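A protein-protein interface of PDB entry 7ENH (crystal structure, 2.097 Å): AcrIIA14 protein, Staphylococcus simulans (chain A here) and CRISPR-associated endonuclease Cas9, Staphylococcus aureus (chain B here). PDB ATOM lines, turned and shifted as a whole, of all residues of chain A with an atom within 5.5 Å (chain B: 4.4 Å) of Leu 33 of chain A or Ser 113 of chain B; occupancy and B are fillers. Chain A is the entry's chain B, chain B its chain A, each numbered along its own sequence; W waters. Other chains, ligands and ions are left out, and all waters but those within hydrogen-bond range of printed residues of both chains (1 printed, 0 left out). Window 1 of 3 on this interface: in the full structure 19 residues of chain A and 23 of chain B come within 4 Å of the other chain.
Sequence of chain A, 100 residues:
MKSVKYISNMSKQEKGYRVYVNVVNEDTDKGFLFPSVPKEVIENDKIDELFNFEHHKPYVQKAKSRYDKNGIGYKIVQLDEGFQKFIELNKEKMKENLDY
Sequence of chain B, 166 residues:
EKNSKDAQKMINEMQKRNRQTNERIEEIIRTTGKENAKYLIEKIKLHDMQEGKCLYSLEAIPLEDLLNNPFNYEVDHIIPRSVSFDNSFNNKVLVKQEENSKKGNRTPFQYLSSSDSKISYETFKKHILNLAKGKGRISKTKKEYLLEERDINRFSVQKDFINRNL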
ATOM      1  N   ASN A   9     -24.649  -0.755  12.020  1.00  0.00           N
ATOM      2  CA  ASN A   9     -24.245   0.639  12.125  1.00  0.00           C
ATOM      3  C   ASN A   9     -25.265   1.513  11.412  1.00  0.00           C
ATOM      4  O   ASN A   9     -25.806   1.122  10.374  1.00  0.00           O
ATOM      5  CB  ASN A   9     -22.850   0.857  11.530  1.00  0.00           C
ATOM      6  CG  ASN A   9     -22.081   1.953  12.238  1.00  0.00           C
ATOM      7  OD1 ASN A   9     -22.649   2.733  13.001  1.00  0.00           O
ATOM      8  ND2 ASN A   9     -20.778   2.016  11.989  1.00  0.00           N
ATOM      9  N   ARG A  18     -27.685   6.490   6.690  1.00  0.00           N
ATOM     10  CA  ARG A  18     -26.703   5.512   6.243  1.00  0.00           C
ATOM     11  C   ARG A  18     -26.833   4.265   7.106  1.00  0.00           C
ATOM     12  O   ARG A  18     -26.845   4.353   8.337  1.00  0.00           O
ATOM     13  CB  ARG A  18     -25.289   6.084   6.330  1.00  0.00           C
ATOM     14  CG  ARG A  18     -24.193   5.087   5.991  1.00  0.00           C
ATOM     15  CD  ARG A  18     -22.862   5.782   5.740  1.00  0.00           C
ATOM     16  NE  ARG A  18     -22.444   6.604   6.873  1.00  0.00           N
ATOM     17  CZ  ARG A  18     -22.289   7.924   6.824  1.00  0.00           C
ATOM     18  NH1 ARG A  18     -22.517   8.581   5.694  1.00  0.00           N
ATOM     19  NH2 ARG A  18     -21.907   8.589   7.906  1.00  0.00           N
ATOM     20  N   VAL A  19     -26.953   3.104   6.465  1.00  0.00           N
ATOM     21  CA  VAL A  19     -27.245   1.855   7.158  1.00  0.00           C
ATOM     22  C   VAL A  19     -26.236   0.797   6.733  1.00  0.00           C
ATOM     23  O   VAL A  19     -25.914   0.674   5.546  1.00  0.00           O
ATOM     24  CB  VAL A  19     -28.687   1.376   6.872  1.00  0.00           C
ATOM     25  CG1 VAL A  19     -28.969   0.059   7.581  1.00  0.00           C
ATOM     26  CG2 VAL A  19     -29.696   2.437   7.293  1.00  0.00           C
ATOM     27  N   TYR A  20     -25.739   0.035   7.704  1.00  0.00           N
ATOM     28  CA  TYR A  20     -24.847  -1.088   7.452  1.00  0.00           C
ATOM     29  C   TYR A  20     -25.476  -2.356   8.010  1.00  0.00           C
ATOM     30  O   TYR A  20     -25.888  -2.390   9.174  1.00  0.00           O
ATOM     31  CB  TYR A  20     -23.469  -0.861   8.077  1.00  0.00           C
ATOM     32  CG  TYR A  20     -22.380  -1.689   7.434  1.00  0.00           C
ATOM     33  CD1 TYR A  20     -22.119  -2.984   7.865  1.00  0.00           C
ATOM     34  CD2 TYR A  20     -21.619  -1.181   6.390  1.00  0.00           C
ATOM     35  CE1 TYR A  20     -21.127  -3.745   7.279  1.00  0.00           C
ATOM     36  CE2 TYR A  20     -20.626  -1.935   5.796  1.00  0.00           C
ATOM     37  CZ  TYR A  20     -20.384  -3.216   6.244  1.00  0.00           C
ATOM     38  OH  TYR A  20     -19.395  -3.971   5.656  1.00  0.00           O
ATOM     39  N   VAL A  21     -25.544  -3.395   7.181  1.00  0.00           N
ATOM     40  CA  VAL A  21     -26.178  -4.656   7.543  1.00  0.00           C
ATOM     41  C   VAL A  21     -25.200  -5.790   7.270  1.00  0.00           C
ATOM     42  O   VAL A  21     -24.626  -5.872   6.178  1.00  0.00           O
ATOM     43  CB  VAL A  21     -27.492  -4.877   6.770  1.00  0.00           C
ATOM     44  CG1 VAL A  21     -27.950  -6.324   6.892  1.00  0.00           C
ATOM     45  CG2 VAL A  21     -28.567  -3.931   7.277  1.00  0.00           C
ATOM     46  N   GLY A  31     -21.075  -7.827   4.596  1.00  0.00           N
ATOM     47  CA  GLY A  31     -21.445  -6.500   5.033  1.00  0.00           C
ATOM     48  C   GLY A  31     -21.948  -5.650   3.885  1.00  0.00           C
ATOM     49  O   GLY A  31     -21.246  -5.453   2.892  1.00  0.00           O
ATOM     50  N   PHE A  32     -23.167  -5.139   4.033  1.00  0.00           N
ATOM     51  CA  PHE A  32     -23.819  -4.326   3.012  1.00  0.00           C
ATOM     52  C   PHE A  32     -23.879  -2.880   3.486  1.00  0.00           C
ATOM     53  O   PHE A  32     -24.467  -2.591   4.534  1.00  0.00           O
ATOM     54  CB  PHE A  32     -25.222  -4.854   2.711  1.00  0.00           C
ATOM     55  CG  PHE A  32     -25.233  -6.162   1.970  1.00  0.00           C
ATOM     56  CD1 PHE A  32     -25.179  -7.364   2.657  1.00  0.00           C
ATOM     57  CD2 PHE A  32     -25.298  -6.188   0.587  1.00  0.00           C
ATOM     58  CE1 PHE A  32     -25.189  -8.568   1.976  1.00  0.00           C
ATOM     59  CE2 PHE A  32     -25.309  -7.389  -0.099  1.00  0.00           C
ATOM     60  CZ  PHE A  32     -25.254  -8.580   0.596  1.00  0.00           C
ATOM     61  N   LEU A  33     -23.277  -1.978   2.713  1.00  0.00           N
ATOM     62  CA  LEU A  33     -23.255  -0.552   3.023  1.00  0.00           C
ATOM     63  C   LEU A  33     -24.342   0.138   2.207  1.00  0.00           C
ATOM     64  O   LEU A  33     -24.222   0.263   0.985  1.00  0.00           O
ATOM     65  CB  LEU A  33     -21.883   0.048   2.719  1.00  0.00           C
ATOM     66  CG  LEU A  33     -21.447   1.366   3.377  1.00  0.00           C
ATOM     67  CD1 LEU A  33     -20.007   1.661   3.009  1.00  0.00           C
ATOM     68  CD2 LEU A  33     -22.329   2.554   3.003  1.00  0.00           C
ATOM     69  N   PHE A  34     -25.391   0.602   2.885  1.00  0.00           N
ATOM     70  CA  PHE A  34     -26.424   1.395   2.239  1.00  0.00           C
ATOM     71  C   PHE A  34     -26.133   2.865   2.488  1.00  0.00           C
ATOM     72  O   PHE A  34     -26.358   3.350   3.608  1.00  0.00           O
ATOM     73  CB  PHE A  34     -27.806   1.023   2.770  1.00  0.00           C
ATOM     74  CG  PHE A  34     -28.213  -0.389   2.460  1.00  0.00           C
ATOM     75  CD1 PHE A  34     -27.832  -1.432   3.288  1.00  0.00           C
ATOM     76  CD2 PHE A  34     -28.977  -0.673   1.339  1.00  0.00           C
ATOM     77  CE1 PHE A  34     -28.204  -2.731   3.006  1.00  0.00           C
ATOM     78  CE2 PHE A  34     -29.352  -1.971   1.052  1.00  0.00           C
ATOM     79  CZ  PHE A  34     -28.965  -3.001   1.885  1.00  0.00           C
ATOM     80  N   PRO A  35     -25.636   3.611   1.497  1.00  0.00           N
ATOM     81  CA  PRO A  35     -25.240   5.002   1.764  1.00  0.00           C
ATOM     82  C   PRO A  35     -26.406   5.915   2.086  1.00  0.00           C
ATOM     83  O   PRO A  35     -26.237   6.858   2.868  1.00  0.00           O
ATOM     84  CB  PRO A  35     -24.547   5.428   0.461  1.00  0.00           C
ATOM     85  CG  PRO A  35     -24.247   4.148  -0.270  1.00  0.00           C
ATOM     86  CD  PRO A  35     -25.351   3.216   0.108  1.00  0.00           C
ATOM     87  N   GLU A  54     -29.978   1.363  -3.113  1.00  0.00           N
ATOM     88  CA  GLU A  54     -28.606   1.162  -3.558  1.00  0.00           C
ATOM     89  C   GLU A  54     -27.694   0.826  -2.387  1.00  0.00           C
ATOM     90  O   GLU A  54     -27.837   1.366  -1.286  1.00  0.00           O
ATOM     91  CB  GLU A  54     -28.100   2.414  -4.276  1.00  0.00           C
ATOM     92  N   HIS A  55     -26.755  -0.083  -2.632  1.00  0.00           N
ATOM     93  CA  HIS A  55     -25.762  -0.447  -1.634  1.00  0.00           C
ATOM     94  C   HIS A  55     -24.479  -0.850  -2.342  1.00  0.00           C
ATOM     95  O   HIS A  55     -24.490  -1.256  -3.506  1.00  0.00           O
ATOM     96  CB  HIS A  55     -26.253  -1.583  -0.725  1.00  0.00           C
ATOM     97  CG  HIS A  55     -26.603  -2.841  -1.460  1.00  0.00           C
ATOM     98  ND1 HIS A  55     -25.651  -3.732  -1.906  1.00  0.00           N
ATOM     99  CD2 HIS A  55     -27.801  -3.361  -1.816  1.00  0.00           C
ATOM    100  CE1 HIS A  55     -26.247  -4.744  -2.511  1.00  0.00           C
ATOM    101  NE2 HIS A  55     -27.552  -4.543  -2.469  1.00  0.00           N
ATOM    102  N   HIS A  56     -23.368  -0.726  -1.623  1.00  0.00           N
ATOM    103  CA  HIS A  56     -22.100  -1.213  -2.138  1.00  0.00           C
ATOM    104  C   HIS A  56     -22.125  -2.735  -2.236  1.00  0.00           C
ATOM    105  O   HIS A  56     -22.949  -3.411  -1.611  1.00  0.00           O
ATOM    106  CB  HIS A  56     -20.942  -0.771  -1.242  1.00  0.00           C
ATOM    107  CG  HIS A  56     -20.665   0.699  -1.287  1.00  0.00           C
ATOM    108  ND1 HIS A  56     -19.431   1.231  -0.982  1.00  0.00           N
ATOM    109  CD2 HIS A  56     -21.461   1.750  -1.598  1.00  0.00           C
ATOM    110  CE1 HIS A  56     -19.478   2.545  -1.106  1.00  0.00           C
ATOM    111  NE2 HIS A  56     -20.699   2.886  -1.478  1.00  0.00           N
ATOM    112  N   PHE B 109     -14.221   4.945   3.984  1.00  0.00           N
ATOM    113  CA  PHE B 109     -15.673   5.058   4.100  1.00  0.00           C
ATOM    114  C   PHE B 109     -16.325   3.689   4.258  1.00  0.00           C
ATOM    115  O   PHE B 109     -17.210   3.505   5.101  1.00  0.00           O
ATOM    116  CB  PHE B 109     -16.231   5.788   2.879  1.00  0.00           C
ATOM    117  CG  PHE B 109     -17.732   5.838   2.830  1.00  0.00           C
ATOM    118  CD1 PHE B 109     -18.448   6.580   3.757  1.00  0.00           C
ATOM    119  CD2 PHE B 109     -18.428   5.150   1.849  1.00  0.00           C
ATOM    120  CE1 PHE B 109     -19.829   6.631   3.708  1.00  0.00           C
ATOM    121  CE2 PHE B 109     -19.809   5.198   1.793  1.00  0.00           C
ATOM    122  CZ  PHE B 109     -20.511   5.939   2.724  1.00  0.00           C
ATOM    123  N   GLN B 110     -15.902   2.713   3.448  1.00  0.00           N
ATOM    124  CA  GLN B 110     -16.457   1.367   3.566  1.00  0.00           C
ATOM    125  C   GLN B 110     -16.073   0.724   4.893  1.00  0.00           C
ATOM    126  O   GLN B 110     -16.856  -0.041   5.470  1.00  0.00           O
ATOM    127  CB  GLN B 110     -15.994   0.499   2.395  1.00  0.00           C
ATOM    128  CG  GLN B 110     -16.626   0.865   1.058  1.00  0.00           C
ATOM    129  CD  GLN B 110     -15.901   0.229  -0.113  1.00  0.00           C
ATOM    130  OE1 GLN B 110     -14.718  -0.099  -0.018  1.00  0.00           O
ATOM    131  NE2 GLN B 110     -16.605   0.056  -1.226  1.00  0.00           N
ATOM    132  N   TYR B 111     -14.872   1.021   5.393  1.00  0.00           N
ATOM    133  CA  TYR B 111     -14.420   0.425   6.645  1.00  0.00           C
ATOM    134  C   TYR B 111     -15.096   1.079   7.845  1.00  0.00           C
ATOM    135  O   TYR B 111     -15.569   0.389   8.755  1.00  0.00           O
ATOM    136  CB  TYR B 111     -12.899   0.535   6.756  1.00  0.00           C
ATOM    137  CG  TYR B 111     -12.356   0.243   8.139  1.00  0.00           C
ATOM    138  CD1 TYR B 111     -12.630  -0.961   8.778  1.00  0.00           C
ATOM    139  CD2 TYR B 111     -11.571   1.173   8.807  1.00  0.00           C
ATOM    140  CE1 TYR B 111     -12.137  -1.229  10.043  1.00  0.00           C
ATOM    141  CE2 TYR B 111     -11.073   0.915  10.070  1.00  0.00           C
ATOM    142  CZ  TYR B 111     -11.359  -0.286  10.683  1.00  0.00           C
ATOM    143  OH  TYR B 111     -10.865  -0.545  11.941  1.00  0.00           O
ATOM    144  N   LEU B 112     -15.150   2.413   7.865  1.00  0.00           N
ATOM    145  CA  LEU B 112     -15.671   3.113   9.033  1.00  0.00           C
ATOM    146  C   LEU B 112     -17.188   3.034   9.134  1.00  0.00           C
ATOM    147  O   LEU B 112     -17.729   3.196  10.232  1.00  0.00           O
ATOM    148  CB  LEU B 112     -15.209   4.569   9.017  1.00  0.00           C
ATOM    149  CG  LEU B 112     -13.686   4.713   9.060  1.00  0.00           C
ATOM    150  CD1 LEU B 112     -13.280   6.115   8.680  1.00  0.00           C
ATOM    151  CD2 LEU B 112     -13.135   4.346  10.429  1.00  0.00           C
ATOM    152  N   SER B 113     -17.883   2.778   8.025  1.00  0.00           N
ATOM    153  CA  SER B 113     -19.316   2.527   8.088  1.00  0.00           C
ATOM    154  C   SER B 113     -19.637   1.119   8.575  1.00  0.00           C
ATOM    155  O   SER B 113     -20.789   0.844   8.921  1.00  0.00           O
ATOM    156  CB  SER B 113     -19.956   2.744   6.714  1.00  0.00           C
ATOM    157  OG  SER B 113     -19.493   3.935   6.113  1.00  0.00           O
ATOM    158  N   SER B 114     -18.648   0.232   8.609  1.00  0.00           N
ATOM    159  CA  SER B 114     -18.852  -1.155   9.004  1.00  0.00           C
ATOM    160  C   SER B 114     -19.101  -1.237  10.510  1.00  0.00           C
ATOM    161  O   SER B 114     -19.344  -0.240  11.197  1.00  0.00           O
ATOM    162  CB  SER B 114     -17.649  -1.996   8.590  1.00  0.00           C
ATOM    163  OG  SER B 114     -16.601  -1.843   9.532  1.00  0.00           O
ATOM    164  N   SER B 115     -19.080  -2.462  11.028  1.00  0.00           N
ATOM    165  CA  SER B 115     -19.053  -2.707  12.461  1.00  0.00           C
ATOM    166  C   SER B 115     -17.645  -2.996  12.958  1.00  0.00           C
ATOM    167  O   SER B 115     -17.464  -3.254  14.151  1.00  0.00           O
ATOM    168  CB  SER B 115     -19.983  -3.873  12.817  1.00  0.00           C
ATOM    169  OG  SER B 115     -19.570  -5.065  12.171  1.00  0.00           O
HETATM  170  O   HOH W   1     -17.693  -2.522   4.432  1.00  0.00           O
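The side-chain amide nitrogen (NE2) of Gln 110 of chain B sits at hydrogen-bond distance from a ring nitrogen (ND1) of His 56 of chain A (3.1 Å). ND2 of Asn 9 of chain A is in hydrogen-bond range of O of Ser 113 of chain B (3.3 Å). The side-chain amide nitrogen of Asn 9 of chain A lies within hydrogen-bond range of the backbone carbonyl oxygen of Ser 114 of chain B, 2.8 Å away.
The side-chain hydroxyl (OG) of Ser 113 of chain B sits at hydrogen-bond distance from the backbone carbonyl oxygen (O) of Phe 109 of chain B. The side-chain hydroxyl (OG) of Ser 114 of chain B sits at hydrogen-bond distance from the backbone carbonyl oxygen (O) of Tyr 111 of chain B (2.6 Å). The backbone carbonyl oxygen (O) of Asn 9 of chain A lies within hydrogen-bond range of the backbone NH (N) of Tyr 20 of chain A (2.9 Å). O of Leu 33 of chain A is in hydrogen-bond range of N of His 56 of chain A, 2.9 Å away.
Asn 9 of chain A touches Leu 112 of chain B. CD of Arg 18 of chain A touches CE1 of Phe 109 of chain B, 3.7 Å away. Arg 18 of chain A touches Ser 113 of chain B. Tyr 20 of chain A touches Ser 113 of chain B. Ser 114 of chain B touches Tyr 20 of chain A (CA to CE2, 3.7 Å). CE2 of Phe 109 of chain B touches CD1 of Leu 33 of chain A (3.7 Å). CD1 of Leu 33 of chain A touches CA of Gln 110 of chain B, at 3.6 Å. Leu 33 of chain A touches Ser 113 of chain B. CE1 of His 56 of chain A touches CE2 of Phe 109 of chain B (3.9 Å).
Leu 33 of chain A touches three residues of chain B. Ser 113 of chain B touches four residues of chain A. Printed residues of chain B within 4 Å of Arg 18 of chain A: Phe 109 and Ser 113. Of the printed residues of chain A, Leu 112 of chain B touches Asn 9 (3.7 Å). Of the printed residues of chain A, Ser 114 of chain B touches Asn 9 and Tyr 20. Printed residues of chain A within 4 Å of Phe 109 of chain B: Arg 18, Leu 33 and His 56. Val 19 of chain A touches none of the printed residues of chain B. The nearest printed residue of chain A that does not touch Ser 113 of chain B is Val 19 of chain A (5.9 Å).
Hydrophobic or aromatic side chains of chain B within 4 Å of the printed part of chain A: Phe 109. Of the 13 printed residues of chain A, 5 touch a printed residue of chain B. Printed residues of chain A that touch a printed residue of chain B: Asn 9, Arg 18, Tyr 20, Leu 33 and His 56. Hydrophobic or aromatic side chains of chain A within 4 Å of the printed part of chain B: Tyr 20, Leu 33 and His 56. Among the printed residues, 12 pairs touch across the chains. Among the printed residues, no Asp or Glu carboxylate lies within 4 Å of a Lys or Arg side-chain nitrogen of the other chain.
Water W1 lies within hydrogen-bond range of the side-chain hydroxyl of Tyr 20 of chain A (2.5 Å) and the backbone carbonyl oxygen of Gln 110 of chain B (2.8 Å).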
